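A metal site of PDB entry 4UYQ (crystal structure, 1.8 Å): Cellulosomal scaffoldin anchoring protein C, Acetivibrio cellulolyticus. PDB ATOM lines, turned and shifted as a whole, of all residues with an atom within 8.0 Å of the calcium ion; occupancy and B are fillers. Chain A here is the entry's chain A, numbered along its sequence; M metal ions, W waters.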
ATOM      1  N   VAL A   4      15.196  18.124 -16.926  1.00  0.00           N
ATOM      2  CA  VAL A   4      15.069  19.530 -17.329  1.00  0.00           C
ATOM      3  C   VAL A   4      14.729  19.620 -18.798  1.00  0.00           C
ATOM      4  O   VAL A   4      15.503  19.195 -19.649  1.00  0.00           O
ATOM      5  CB  VAL A   4      16.362  20.302 -17.002  1.00  0.00           C
ATOM      6  CG1 VAL A   4      16.240  21.762 -17.398  1.00  0.00           C
ATOM      7  CG2 VAL A   4      16.729  20.134 -15.508  1.00  0.00           C
ATOM      8  N   ASP A   5      13.539  20.126 -19.086  1.00  0.00           N
ATOM      9  CA  ASP A   5      12.965  20.230 -20.452  1.00  0.00           C
ATOM     10  C   ASP A   5      12.895  21.669 -20.927  1.00  0.00           C
ATOM     11  O   ASP A   5      12.274  22.554 -20.279  1.00  0.00           O
ATOM     12  CB  ASP A   5      11.564  19.653 -20.463  1.00  0.00           C
ATOM     13  CG  ASP A   5      10.893  19.733 -21.821  1.00  0.00           C
ATOM     14  OD1 ASP A   5      11.455  19.080 -22.743  1.00  0.00           O
ATOM     15  OD2 ASP A   5       9.792  20.399 -21.928  1.00  0.00           O
ATOM     16  N   ILE A   6      13.564  21.923 -21.996  1.00  0.00           N
ATOM     17  CA  ILE A   6      13.289  23.122 -22.798  1.00  0.00           C
ATOM     18  C   ILE A   6      12.069  22.794 -23.652  1.00  0.00           C
ATOM     19  O   ILE A   6      12.097  21.835 -24.418  1.00  0.00           O
ATOM     20  CB  ILE A   6      14.469  23.493 -23.717  1.00  0.00           C
ATOM     21  CG1 ILE A   6      15.724  23.685 -22.902  1.00  0.00           C
ATOM     22  CG2 ILE A   6      14.071  24.695 -24.587  1.00  0.00           C
ATOM     23  CD1 ILE A   6      16.951  23.917 -23.740  1.00  0.00           C
ATOM     24  N   GLY A   7      10.989  23.536 -23.478  1.00  0.00           N
ATOM     25  CA  GLY A   7       9.759  23.247 -24.197  1.00  0.00           C
ATOM     26  C   GLY A   7       9.783  23.473 -25.683  1.00  0.00           C
ATOM     27  O   GLY A   7      10.662  24.210 -26.183  1.00  0.00           O
ATOM     28  N   SER A   8       8.898  22.757 -26.399  1.00  0.00           N
ATOM     29  CA  SER A   8       8.797  23.018 -27.828  1.00  0.00           C
ATOM     30  C   SER A   8       7.479  23.704 -28.123  1.00  0.00           C
ATOM     31  O   SER A   8       6.529  23.565 -27.343  1.00  0.00           O
ATOM     32  CB  SER A   8       8.887  21.706 -28.594  1.00  0.00           C
ATOM     33  OG  SER A   8      10.193  21.145 -28.485  1.00  0.00           O
ATOM     34  N   VAL A  19       8.601  29.536 -24.687  1.00  0.00           N
ATOM     35  CA  VAL A  19       9.354  28.286 -24.429  1.00  0.00           C
ATOM     36  C   VAL A  19       9.532  28.106 -22.882  1.00  0.00           C
ATOM     37  O   VAL A  19      10.402  28.728 -22.280  1.00  0.00           O
ATOM     38  CB  VAL A  19      10.689  28.367 -25.125  1.00  0.00           C
ATOM     39  CG1 VAL A  19      11.594  27.184 -24.727  1.00  0.00           C
ATOM     40  CG2 VAL A  19      10.467  28.391 -26.655  1.00  0.00           C
ATOM     41  N   PRO A  20       8.681  27.330 -22.245  1.00  0.00           N
ATOM     42  CA  PRO A  20       8.888  27.133 -20.815  1.00  0.00           C
ATOM     43  C   PRO A  20      10.047  26.166 -20.497  1.00  0.00           C
ATOM     44  O   PRO A  20      10.349  25.241 -21.262  1.00  0.00           O
ATOM     45  CB  PRO A  20       7.564  26.503 -20.366  1.00  0.00           C
ATOM     46  CG  PRO A  20       7.115  25.766 -21.545  1.00  0.00           C
ATOM     47  CD  PRO A  20       7.428  26.699 -22.682  1.00  0.00           C
ATOM     48  N   ILE A 112      16.667  25.043 -29.810  1.00  0.00           N
ATOM     49  CA  ILE A 112      17.000  25.786 -28.587  1.00  0.00           C
ATOM     50  C   ILE A 112      17.707  24.783 -27.707  1.00  0.00           C
ATOM     51  O   ILE A 112      17.090  23.823 -27.225  1.00  0.00           O
ATOM     52  CB  ILE A 112      15.709  26.341 -27.904  1.00  0.00           C
ATOM     53  CG1 ILE A 112      14.828  27.128 -28.888  1.00  0.00           C
ATOM     54  CG2 ILE A 112      16.042  27.233 -26.716  1.00  0.00           C
ATOM     55  CD1 ILE A 112      15.517  28.269 -29.574  1.00  0.00           C
ATOM     56  N   TYR A 134      18.629  16.318 -19.677  1.00  0.00           N
ATOM     57  CA  TYR A 134      18.181  17.477 -20.343  1.00  0.00           C
ATOM     58  C   TYR A 134      17.470  17.067 -21.657  1.00  0.00           C
ATOM     59  O   TYR A 134      17.839  16.063 -22.270  1.00  0.00           O
ATOM     60  CB  TYR A 134      19.376  18.297 -20.737  1.00  0.00           C
ATOM     61  CG  TYR A 134      20.062  18.844 -19.506  1.00  0.00           C
ATOM     62  CD1 TYR A 134      19.578  19.984 -18.870  1.00  0.00           C
ATOM     63  CD2 TYR A 134      21.177  18.240 -18.994  1.00  0.00           C
ATOM     64  CE1 TYR A 134      20.195  20.501 -17.726  1.00  0.00           C
ATOM     65  CE2 TYR A 134      21.823  18.758 -17.841  1.00  0.00           C
ATOM     66  CZ  TYR A 134      21.337  19.899 -17.246  1.00  0.00           C
ATOM     67  OH  TYR A 134      21.916  20.366 -16.126  1.00  0.00           O
ATOM     68  N   ASN A 135      16.449  17.776 -22.017  1.00  0.00           N
ATOM     69  CA  ASN A 135      15.794  17.599 -23.343  1.00  0.00           C
ATOM     70  C   ASN A 135      15.647  18.958 -24.036  1.00  0.00           C
ATOM     71  O   ASN A 135      14.900  19.831 -23.549  1.00  0.00           O
ATOM     72  CB  ASN A 135      14.454  16.987 -23.138  1.00  0.00           C
ATOM     73  CG  ASN A 135      13.722  16.698 -24.491  1.00  0.00           C
ATOM     74  OD1 ASN A 135      12.921  17.457 -24.900  1.00  0.00           O
ATOM     75  ND2 ASN A 135      13.974  15.571 -25.082  1.00  0.00           N
ATOM     76  N   ASP A 136      16.298  19.141 -25.199  1.00  0.00           N
ATOM     77  CA  ASP A 136      16.282  20.399 -25.858  1.00  0.00           C
ATOM     78  C   ASP A 136      14.920  20.723 -26.539  1.00  0.00           C
ATOM     79  O   ASP A 136      14.018  19.895 -26.571  1.00  0.00           O
ATOM     80  CB  ASP A 136      17.400  20.502 -26.883  1.00  0.00           C
ATOM     81  CG  ASP A 136      18.820  20.511 -26.243  1.00  0.00           C
ATOM     82  OD1 ASP A 136      18.999  20.937 -25.098  1.00  0.00           O
ATOM     83  OD2 ASP A 136      19.765  20.122 -26.947  1.00  0.00           O
ATOM     84  N   GLY A 137      14.817  21.925 -27.062  1.00  0.00           N
ATOM     85  CA  GLY A 137      13.552  22.529 -27.511  1.00  0.00           C
ATOM     86  C   GLY A 137      13.553  22.788 -28.986  1.00  0.00           C
ATOM     87  O   GLY A 137      14.620  22.917 -29.587  1.00  0.00           O
ATOM     88  N   LYS A 138      12.357  22.794 -29.558  1.00  0.00           N
ATOM     89  CA  LYS A 138      12.161  22.919 -30.990  1.00  0.00           C
ATOM     90  C   LYS A 138      11.189  24.037 -31.162  1.00  0.00           C
ATOM     91  O   LYS A 138      10.172  24.098 -30.459  1.00  0.00           O
ATOM     92  CB  LYS A 138      11.510  21.657 -31.568  1.00  0.00           C
ATOM     93  CG  LYS A 138      12.358  20.394 -31.513  1.00  0.00           C
ATOM     94  CD  LYS A 138      11.483  19.211 -31.706  1.00  0.00           C
ATOM     95  CE  LYS A 138      12.158  17.869 -31.488  1.00  0.00           C
ATOM     96  NZ  LYS A 138      11.165  16.765 -31.740  1.00  0.00           N
HETATM   97 CA    CA M   1      12.334  19.569 -24.854  1.00  0.00          CA
HETATM   98  O   HOH W   1      10.486  19.370 -26.392  1.00  0.00           O
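N of Asn 135 lies within hydrogen-bond range of O of Val 4 (2.9 Å).
Of the 13 residues printed, 4 come within 4 Å of the calcium ion. The nearest printed residue that does not touch the calcium ion is Gly 137 (4.1 Å).
The calcium ion is bound by OD1 of Asn 135 (2.2 Å), O of Ile 6 (2.3 Å), OD1 of Asp 5 (2.3 Å), water W1 (2.4 Å), O of Asp 136 (2.4 Å) and O of Asn 135 (2.9 Å).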
